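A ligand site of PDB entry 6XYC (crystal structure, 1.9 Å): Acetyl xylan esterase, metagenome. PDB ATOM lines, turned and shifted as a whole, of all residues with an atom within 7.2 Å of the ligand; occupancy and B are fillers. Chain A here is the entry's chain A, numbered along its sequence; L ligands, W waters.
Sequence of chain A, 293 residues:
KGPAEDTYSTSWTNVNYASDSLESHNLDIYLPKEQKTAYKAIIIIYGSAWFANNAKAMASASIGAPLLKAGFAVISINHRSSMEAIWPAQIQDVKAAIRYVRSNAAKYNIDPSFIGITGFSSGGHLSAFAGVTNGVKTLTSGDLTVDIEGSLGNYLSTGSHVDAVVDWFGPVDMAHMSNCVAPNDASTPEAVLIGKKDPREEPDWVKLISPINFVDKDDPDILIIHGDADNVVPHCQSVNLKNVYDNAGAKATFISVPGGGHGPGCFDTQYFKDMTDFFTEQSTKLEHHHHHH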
ATOM      1  N   TYR A  46      23.936 -15.599  -1.515  1.00  0.00           N
ATOM      2  CA  TYR A  46      24.988 -15.065  -2.368  1.00  0.00           C
ATOM      3  C   TYR A  46      25.565 -16.151  -3.275  1.00  0.00           C
ATOM      4  O   TYR A  46      25.443 -17.356  -3.005  1.00  0.00           O
ATOM      5  CB  TYR A  46      26.123 -14.479  -1.526  1.00  0.00           C
ATOM      6  CG  TYR A  46      26.657 -15.442  -0.480  1.00  0.00           C
ATOM      7  CD1 TYR A  46      26.272 -15.324   0.854  1.00  0.00           C
ATOM      8  CD2 TYR A  46      27.531 -16.470  -0.816  1.00  0.00           C
ATOM      9  CE1 TYR A  46      26.743 -16.205   1.812  1.00  0.00           C
ATOM     10  CE2 TYR A  46      28.017 -17.354   0.143  1.00  0.00           C
ATOM     11  CZ  TYR A  46      27.613 -17.215   1.453  1.00  0.00           C
ATOM     12  OH  TYR A  46      28.080 -18.084   2.417  1.00  0.00           O
ATOM     13  N   GLY A  47      26.224 -15.712  -4.336  1.00  0.00           N
ATOM     14  CA  GLY A  47      27.047 -16.569  -5.164  1.00  0.00           C
ATOM     15  C   GLY A  47      28.509 -16.420  -4.821  1.00  0.00           C
ATOM     16  O   GLY A  47      28.986 -15.338  -4.477  1.00  0.00           O
ATOM     17  N   SER A  48      29.242 -17.534  -4.922  1.00  0.00           N
ATOM     18  CA  SER A  48      30.633 -17.557  -4.506  1.00  0.00           C
ATOM     19  C   SER A  48      31.361 -18.819  -4.966  1.00  0.00           C
ATOM     20  O   SER A  48      32.398 -19.175  -4.401  1.00  0.00           O
ATOM     21  CB  SER A  48      30.738 -17.470  -2.987  1.00  0.00           C
ATOM     22  OG  SER A  48      30.343 -18.700  -2.386  1.00  0.00           O
ATOM     23  N   ALA A  49      30.813 -19.503  -5.980  1.00  0.00           N
ATOM     24  CA  ALA A  49      31.327 -20.819  -6.386  1.00  0.00           C
ATOM     25  C   ALA A  49      31.406 -21.754  -5.177  1.00  0.00           C
ATOM     26  O   ALA A  49      32.290 -22.605  -5.087  1.00  0.00           O
ATOM     27  CB  ALA A  49      32.688 -20.695  -7.079  1.00  0.00           C
ATOM     28  N   TRP A  50      30.488 -21.561  -4.227  1.00  0.00           N
ATOM     29  CA  TRP A  50      30.378 -22.319  -2.973  1.00  0.00           C
ATOM     30  C   TRP A  50      31.526 -22.067  -1.995  1.00  0.00           C
ATOM     31  O   TRP A  50      31.587 -22.722  -0.950  1.00  0.00           O
ATOM     32  CB  TRP A  50      30.255 -23.830  -3.233  1.00  0.00           C
ATOM     33  CG  TRP A  50      29.055 -24.197  -4.067  1.00  0.00           C
ATOM     34  CD1 TRP A  50      27.752 -24.148  -3.689  1.00  0.00           C
ATOM     35  CD2 TRP A  50      29.068 -24.676  -5.418  1.00  0.00           C
ATOM     36  NE1 TRP A  50      26.935 -24.554  -4.711  1.00  0.00           N
ATOM     37  CE2 TRP A  50      27.718 -24.881  -5.791  1.00  0.00           C
ATOM     38  CE3 TRP A  50      30.073 -24.935  -6.347  1.00  0.00           C
ATOM     39  CZ2 TRP A  50      27.367 -25.339  -7.059  1.00  0.00           C
ATOM     40  CZ3 TRP A  50      29.715 -25.390  -7.607  1.00  0.00           C
ATOM     41  CH2 TRP A  50      28.375 -25.582  -7.947  1.00  0.00           C
ATOM     42  N   PHE A  51      32.419 -21.120  -2.291  1.00  0.00           N
ATOM     43  CA  PHE A  51      33.623 -20.953  -1.489  1.00  0.00           C
ATOM     44  C   PHE A  51      33.403 -20.061  -0.273  1.00  0.00           C
ATOM     45  O   PHE A  51      34.131 -20.187   0.719  1.00  0.00           O
ATOM     46  CB  PHE A  51      34.772 -20.363  -2.309  1.00  0.00           C
ATOM     47  CG  PHE A  51      35.428 -21.337  -3.261  1.00  0.00           C
ATOM     48  CD1 PHE A  51      35.721 -22.628  -2.874  1.00  0.00           C
ATOM     49  CD2 PHE A  51      35.767 -20.924  -4.540  1.00  0.00           C
ATOM     50  CE1 PHE A  51      36.314 -23.518  -3.756  1.00  0.00           C
ATOM     51  CE2 PHE A  51      36.363 -21.796  -5.425  1.00  0.00           C
ATOM     52  CZ  PHE A  51      36.647 -23.094  -5.029  1.00  0.00           C
ATOM     53  N   PHE A 120      22.079 -16.064  -6.565  1.00  0.00           N
ATOM     54  CA  PHE A 120      22.786 -15.939  -7.836  1.00  0.00           C
ATOM     55  C   PHE A 120      24.012 -16.854  -7.880  1.00  0.00           C
ATOM     56  O   PHE A 120      24.676 -17.045  -6.857  1.00  0.00           O
ATOM     57  CB  PHE A 120      23.166 -14.450  -8.134  1.00  0.00           C
ATOM     58  CG  PHE A 120      23.818 -13.709  -6.995  1.00  0.00           C
ATOM     59  CD1 PHE A 120      23.053 -13.108  -6.000  1.00  0.00           C
ATOM     60  CD2 PHE A 120      25.189 -13.552  -6.958  1.00  0.00           C
ATOM     61  CE1 PHE A 120      23.658 -12.424  -4.974  1.00  0.00           C
ATOM     62  CE2 PHE A 120      25.787 -12.867  -5.938  1.00  0.00           C
ATOM     63  CZ  PHE A 120      25.023 -12.298  -4.947  1.00  0.00           C
ATOM     64  N   SER A 121      24.298 -17.406  -9.070  1.00  0.00           N
ATOM     65  CA  SER A 121      25.316 -18.426  -9.282  1.00  0.00           C
ATOM     66  C   SER A 121      25.120 -19.513  -8.234  1.00  0.00           C
ATOM     67  O   SER A 121      24.053 -20.139  -8.181  1.00  0.00           O
ATOM     68  CB  SER A 121      26.724 -17.824  -9.239  1.00  0.00           C
ATOM     69  OG  SER A 121      27.626 -18.678  -9.933  1.00  0.00           O
ATOM     70  N   SER A 122      26.136 -19.790  -7.414  1.00  0.00           N
ATOM     71  CA  SER A 122      26.046 -20.928  -6.518  1.00  0.00           C
ATOM     72  C   SER A 122      24.880 -20.757  -5.560  1.00  0.00           C
ATOM     73  O   SER A 122      24.314 -21.757  -5.100  1.00  0.00           O
ATOM     74  CB  SER A 122      27.355 -21.146  -5.747  1.00  0.00           C
ATOM     75  OG  SER A 122      27.778 -20.004  -5.032  1.00  0.00           O
ATOM     76  N   GLY A 123      24.473 -19.520  -5.282  1.00  0.00           N
ATOM     77  CA  GLY A 123      23.258 -19.302  -4.500  1.00  0.00           C
ATOM     78  C   GLY A 123      21.994 -19.627  -5.266  1.00  0.00           C
ATOM     79  O   GLY A 123      20.989 -20.040  -4.679  1.00  0.00           O
ATOM     80  N   GLY A 124      22.018 -19.425  -6.583  1.00  0.00           N
ATOM     81  CA  GLY A 124      20.921 -19.894  -7.413  1.00  0.00           C
ATOM     82  C   GLY A 124      20.870 -21.405  -7.490  1.00  0.00           C
ATOM     83  O   GLY A 124      19.782 -21.991  -7.556  1.00  0.00           O
ATOM     84  N   HIS A 125      22.032 -22.054  -7.481  1.00  0.00           N
ATOM     85  CA  HIS A 125      22.098 -23.516  -7.403  1.00  0.00           C
ATOM     86  C   HIS A 125      21.446 -24.019  -6.112  1.00  0.00           C
ATOM     87  O   HIS A 125      20.631 -24.942  -6.149  1.00  0.00           O
ATOM     88  CB  HIS A 125      23.556 -23.948  -7.492  1.00  0.00           C
ATOM     89  CG  HIS A 125      23.823 -25.329  -6.971  1.00  0.00           C
ATOM     90  ND1 HIS A 125      24.144 -25.578  -5.649  1.00  0.00           N
ATOM     91  CD2 HIS A 125      23.852 -26.518  -7.605  1.00  0.00           C
ATOM     92  CE1 HIS A 125      24.341 -26.881  -5.494  1.00  0.00           C
ATOM     93  NE2 HIS A 125      24.165 -27.473  -6.662  1.00  0.00           N
ATOM     94  N   PHE A 169      21.238 -17.215 -12.881  1.00  0.00           N
ATOM     95  CA  PHE A 169      22.401 -17.838 -13.539  1.00  0.00           C
ATOM     96  C   PHE A 169      23.129 -18.849 -12.634  1.00  0.00           C
ATOM     97  O   PHE A 169      24.344 -18.785 -12.446  1.00  0.00           O
ATOM     98  CB  PHE A 169      23.381 -16.788 -14.086  1.00  0.00           C
ATOM     99  CG  PHE A 169      23.679 -15.613 -13.144  1.00  0.00           C
ATOM    100  CD1 PHE A 169      23.001 -14.407 -13.277  1.00  0.00           C
ATOM    101  CD2 PHE A 169      24.683 -15.694 -12.185  1.00  0.00           C
ATOM    102  CE1 PHE A 169      23.273 -13.332 -12.429  1.00  0.00           C
ATOM    103  CE2 PHE A 169      24.953 -14.628 -11.336  1.00  0.00           C
ATOM    104  CZ  PHE A 169      24.257 -13.439 -11.466  1.00  0.00           C
ATOM    105  N   GLY A 170      22.392 -19.839 -12.128  1.00  0.00           N
ATOM    106  CA  GLY A 170      22.960 -20.856 -11.275  1.00  0.00           C
ATOM    107  C   GLY A 170      23.502 -22.042 -12.055  1.00  0.00           C
ATOM    108  O   GLY A 170      22.944 -22.448 -13.082  1.00  0.00           O
ATOM    109  N   PRO A 171      24.631 -22.595 -11.609  1.00  0.00           N
ATOM    110  CA  PRO A 171      25.142 -23.857 -12.150  1.00  0.00           C
ATOM    111  C   PRO A 171      24.307 -25.017 -11.599  1.00  0.00           C
ATOM    112  O   PRO A 171      24.369 -25.303 -10.402  1.00  0.00           O
ATOM    113  CB  PRO A 171      26.589 -23.894 -11.676  1.00  0.00           C
ATOM    114  CG  PRO A 171      26.566 -23.172 -10.370  1.00  0.00           C
ATOM    115  CD  PRO A 171      25.504 -22.088 -10.508  1.00  0.00           C
ATOM    116  N   MET A 174      25.867 -30.040 -13.614  1.00  0.00           N
ATOM    117  CA  MET A 174      27.324 -30.143 -13.624  1.00  0.00           C
ATOM    118  C   MET A 174      27.819 -31.273 -14.524  1.00  0.00           C
ATOM    119  O   MET A 174      29.029 -31.322 -14.806  1.00  0.00           O
ATOM    120  CB  MET A 174      27.851 -30.327 -12.207  1.00  0.00           C
ATOM    121  CG  MET A 174      28.333 -29.032 -11.569  1.00  0.00           C
ATOM    122  SD  MET A 174      27.089 -27.731 -11.510  1.00  0.00           S
ATOM    123  CE  MET A 174      26.049 -28.305 -10.160  1.00  0.00           C
ATOM    124  N   MET A 177      28.888 -28.942 -17.774  1.00  0.00           N
ATOM    125  CA  MET A 177      29.467 -27.640 -17.475  1.00  0.00           C
ATOM    126  C   MET A 177      30.594 -27.278 -18.429  1.00  0.00           C
ATOM    127  O   MET A 177      30.676 -26.130 -18.877  1.00  0.00           O
ATOM    128  CB  MET A 177      29.971 -27.610 -16.035  1.00  0.00           C
ATOM    129  CG  MET A 177      30.358 -26.215 -15.551  1.00  0.00           C
ATOM    130  SD  MET A 177      28.967 -25.076 -15.610  1.00  0.00           S
ATOM    131  CE  MET A 177      28.028 -25.608 -14.189  1.00  0.00           C
ATOM    132  N   SER A 178      31.460 -28.229 -18.739  1.00  0.00           N
ATOM    133  CA  SER A 178      32.631 -27.975 -19.587  1.00  0.00           C
ATOM    134  C   SER A 178      32.190 -28.010 -21.050  1.00  0.00           C
ATOM    135  O   SER A 178      31.655 -29.024 -21.515  1.00  0.00           O
ATOM    136  CB  SER A 178      33.724 -29.008 -19.321  1.00  0.00           C
ATOM    137  OG  SER A 178      34.771 -28.907 -20.269  1.00  0.00           O
ATOM    138  N   ASN A 184      33.455 -30.961 -15.515  1.00  0.00           N
ATOM    139  CA  ASN A 184      34.732 -30.288 -15.364  1.00  0.00           C
ATOM    140  C   ASN A 184      35.750 -31.221 -14.689  1.00  0.00           C
ATOM    141  O   ASN A 184      35.419 -32.306 -14.215  1.00  0.00           O
ATOM    142  CB  ASN A 184      34.576 -29.008 -14.541  1.00  0.00           C
ATOM    143  CG  ASN A 184      34.270 -27.797 -15.402  1.00  0.00           C
ATOM    144  OD1 ASN A 184      34.858 -27.611 -16.465  1.00  0.00           O
ATOM    145  ND2 ASN A 184      33.365 -26.959 -14.920  1.00  0.00           N
ATOM    146  N   THR A 188      38.215 -27.488 -10.447  1.00  0.00           N
ATOM    147  CA  THR A 188      37.118 -26.541 -10.517  1.00  0.00           C
ATOM    148  C   THR A 188      36.348 -26.475  -9.212  1.00  0.00           C
ATOM    149  O   THR A 188      36.520 -27.305  -8.318  1.00  0.00           O
ATOM    150  CB  THR A 188      36.184 -26.920 -11.661  1.00  0.00           C
ATOM    151  OG1 THR A 188      35.674 -28.232 -11.461  1.00  0.00           O
ATOM    152  CG2 THR A 188      36.922 -26.861 -12.996  1.00  0.00           C
ATOM    153  N   PRO A 189      35.477 -25.472  -9.065  1.00  0.00           N
ATOM    154  CA  PRO A 189      34.735 -25.334  -7.798  1.00  0.00           C
ATOM    155  C   PRO A 189      33.845 -26.521  -7.449  1.00  0.00           C
ATOM    156  O   PRO A 189      33.734 -26.878  -6.268  1.00  0.00           O
ATOM    157  CB  PRO A 189      33.922 -24.050  -8.002  1.00  0.00           C
ATOM    158  CG  PRO A 189      34.786 -23.228  -8.974  1.00  0.00           C
ATOM    159  CD  PRO A 189      35.339 -24.284  -9.927  1.00  0.00           C
ATOM    160  N   GLU A 190      33.181 -27.137  -8.440  1.00  0.00           N
ATOM    161  CA  GLU A 190      32.348 -28.290  -8.133  1.00  0.00           C
ATOM    162  C   GLU A 190      33.181 -29.472  -7.672  1.00  0.00           C
ATOM    163  O   GLU A 190      32.698 -30.301  -6.885  1.00  0.00           O
ATOM    164  CB  GLU A 190      31.498 -28.682  -9.334  1.00  0.00           C
ATOM    165  CG  GLU A 190      32.280 -28.950 -10.593  1.00  0.00           C
ATOM    166  CD  GLU A 190      32.232 -27.782 -11.547  1.00  0.00           C
ATOM    167  OE1 GLU A 190      31.792 -27.951 -12.707  1.00  0.00           O
ATOM    168  OE2 GLU A 190      32.634 -26.677 -11.140  1.00  0.00           O
ATOM    169  N   ALA A 191      34.431 -29.574  -8.141  1.00  0.00           N
ATOM    170  CA  ALA A 191      35.326 -30.620  -7.648  1.00  0.00           C
ATOM    171  C   ALA A 191      35.577 -30.452  -6.156  1.00  0.00           C
ATOM    172  O   ALA A 191      35.564 -31.418  -5.398  1.00  0.00           O
ATOM    173  CB  ALA A 191      36.652 -30.603  -8.427  1.00  0.00           C
ATOM    174  N   VAL A 232      30.997 -17.106 -16.985  1.00  0.00           N
ATOM    175  CA  VAL A 232      31.396 -17.805 -15.770  1.00  0.00           C
ATOM    176  C   VAL A 232      30.575 -19.084 -15.625  1.00  0.00           C
ATOM    177  O   VAL A 232      31.130 -20.184 -15.503  1.00  0.00           O
ATOM    178  CB  VAL A 232      31.257 -16.906 -14.535  1.00  0.00           C
ATOM    179  CG1 VAL A 232      31.620 -17.674 -13.275  1.00  0.00           C
ATOM    180  CG2 VAL A 232      32.133 -15.678 -14.667  1.00  0.00           C
ATOM    181  N   VAL A 233      29.247 -18.945 -15.615  1.00  0.00           N
ATOM    182  CA  VAL A 233      28.333 -20.081 -15.694  1.00  0.00           C
ATOM    183  C   VAL A 233      27.609 -19.981 -17.032  1.00  0.00           C
ATOM    184  O   VAL A 233      26.911 -18.992 -17.272  1.00  0.00           O
ATOM    185  CB  VAL A 233      27.327 -20.078 -14.525  1.00  0.00           C
ATOM    186  CG1 VAL A 233      26.364 -21.245 -14.684  1.00  0.00           C
ATOM    187  CG2 VAL A 233      28.062 -20.160 -13.196  1.00  0.00           C
ATOM    188  N   PRO A 234      27.738 -20.956 -17.922  1.00  0.00           N
ATOM    189  CA  PRO A 234      27.186 -20.789 -19.272  1.00  0.00           C
ATOM    190  C   PRO A 234      25.656 -20.800 -19.296  1.00  0.00           C
ATOM    191  O   PRO A 234      24.997 -21.538 -18.553  1.00  0.00           O
ATOM    192  CB  PRO A 234      27.766 -21.963 -20.061  1.00  0.00           C
ATOM    193  CG  PRO A 234      28.153 -22.982 -19.027  1.00  0.00           C
ATOM    194  CD  PRO A 234      28.522 -22.214 -17.799  1.00  0.00           C
ATOM    195  N   HIS A 262      27.698 -12.230 -15.942  1.00  0.00           N
ATOM    196  CA  HIS A 262      27.503 -12.940 -14.685  1.00  0.00           C
ATOM    197  C   HIS A 262      27.109 -11.947 -13.584  1.00  0.00           C
ATOM    198  O   HIS A 262      27.795 -11.774 -12.573  1.00  0.00           O
ATOM    199  CB  HIS A 262      28.768 -13.720 -14.348  1.00  0.00           C
ATOM    200  CG  HIS A 262      28.571 -14.849 -13.387  1.00  0.00           C
ATOM    201  ND1 HIS A 262      27.761 -15.938 -13.651  1.00  0.00           N
ATOM    202  CD2 HIS A 262      29.132 -15.088 -12.177  1.00  0.00           C
ATOM    203  CE1 HIS A 262      27.794 -16.776 -12.632  1.00  0.00           C
ATOM    204  NE2 HIS A 262      28.622 -16.283 -11.714  1.00  0.00           N
HETATM  205  C1  LIG L   1      31.840 -20.658 -11.023  1.00  0.00           C
HETATM  206  C2  LIG L   1      31.022 -19.674 -10.547  1.00  0.00           C
HETATM  207  C3  LIG L   1      29.899 -20.019  -9.852  1.00  0.00           C
HETATM  208  S1  LIG L   1      28.926 -18.719  -9.242  1.00  0.00           S
HETATM  209  O1  LIG L   1      28.839 -18.806  -7.767  1.00  0.00           O
HETATM  210  O2  LIG L   1      29.663 -17.466  -9.389  1.00  0.00           O
HETATM  211  C4  LIG L   1      29.578 -21.322  -9.614  1.00  0.00           C
HETATM  212  C5  LIG L   1      30.409 -22.309 -10.090  1.00  0.00           C
HETATM  213  C6  LIG L   1      31.537 -21.976 -10.791  1.00  0.00           C
HETATM  214  C7  LIG L   1      32.488 -23.090 -11.353  1.00  0.00           C
HETATM  215  C8  LIG L   1      31.689 -24.059 -12.261  1.00  0.00           C
HETATM  216  N1  LIG L   1      32.641 -24.808 -13.012  1.00  0.00           N
HETATM  217  O   HOH W   1      32.414 -17.401  -9.469  1.00  0.00           O
HETATM  218  O   HOH W   2      33.388 -24.208 -15.372  1.00  0.00           O
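Water W2 lies within hydrogen-bond range of N1 of the ligand and ND2 of Asn 184.
The side-chain hydroxyl (OG) of Ser 121 is bonded to a sulfur (S1) of the ligand, 1.5 Å away.
The side-chain carboxylate (OE2) of Glu 190 is in salt-bridge range of a nitrogen (N1) of the ligand, at 2.6 Å.
The backbone NH (N) of Ala 49 sits at hydrogen-bond distance from an oxygen (O1) of the ligand (2.8 Å).
A ring nitrogen (NE2) of His 262 sits at hydrogen-bond distance from an oxygen (O2) of the ligand, at 2.8 Å.
An oxygen (O1) of the ligand lies within hydrogen-bond range of the backbone NH of Ser 122.
OG of Ser 122 lies within hydrogen-bond range of O1 of the ligand, 3.2 Å away.
The side-chain amide nitrogen (ND2) of Asn 184 lies close to a nitrogen (N1) of the ligand (3.0 Å).
The backbone NH (N) of Ser 48 sits at hydrogen-bond distance from an oxygen (O1) of the ligand, 3.1 Å away.
A ring nitrogen (NE2) of His 262 is in hydrogen-bond range of the side-chain hydroxyl (OG) of Ser 121.
The side-chain carboxylate (OE1) of Glu 190 lies within hydrogen-bond range of the side-chain amide nitrogen (ND2) of Asn 184, 2.9 Å away.
The side-chain hydroxyl (OG1) of Thr 188 sits at hydrogen-bond distance from the side-chain carboxylate (OE2) of Glu 190, 3.4 Å away.
The backbone NH of Ala 49 lies within hydrogen-bond range of the side-chain hydroxyl of Ser 122 (3.2 Å).
The side-chain hydroxyl of Ser 122 lies within hydrogen-bond range of the backbone NH of Ser 48, 2.9 Å away.
The side-chain hydroxyl (OG) of Ser 122 is in hydrogen-bond range of the backbone NH (N) of Trp 50.
OG of Ser 48 sits close to N of Trp 50.
O of Phe 120 lies close to N of Gly 47, 3.2 Å away.
Gly 47 touches the ligand.
Pro 171 touches the ligand.
Met 177 touches the ligand.
Pro 189 touches the ligand (CG to C7, 3.3 Å).
Val 232 touches the ligand.
Val 233 touches the ligand (CG2 to C3, 3.8 Å).
Of the 27 residues printed, 13 come within 4 Å of the ligand.
The nearest printed residue that does not touch the ligand is Trp 50 (4.02 Å).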
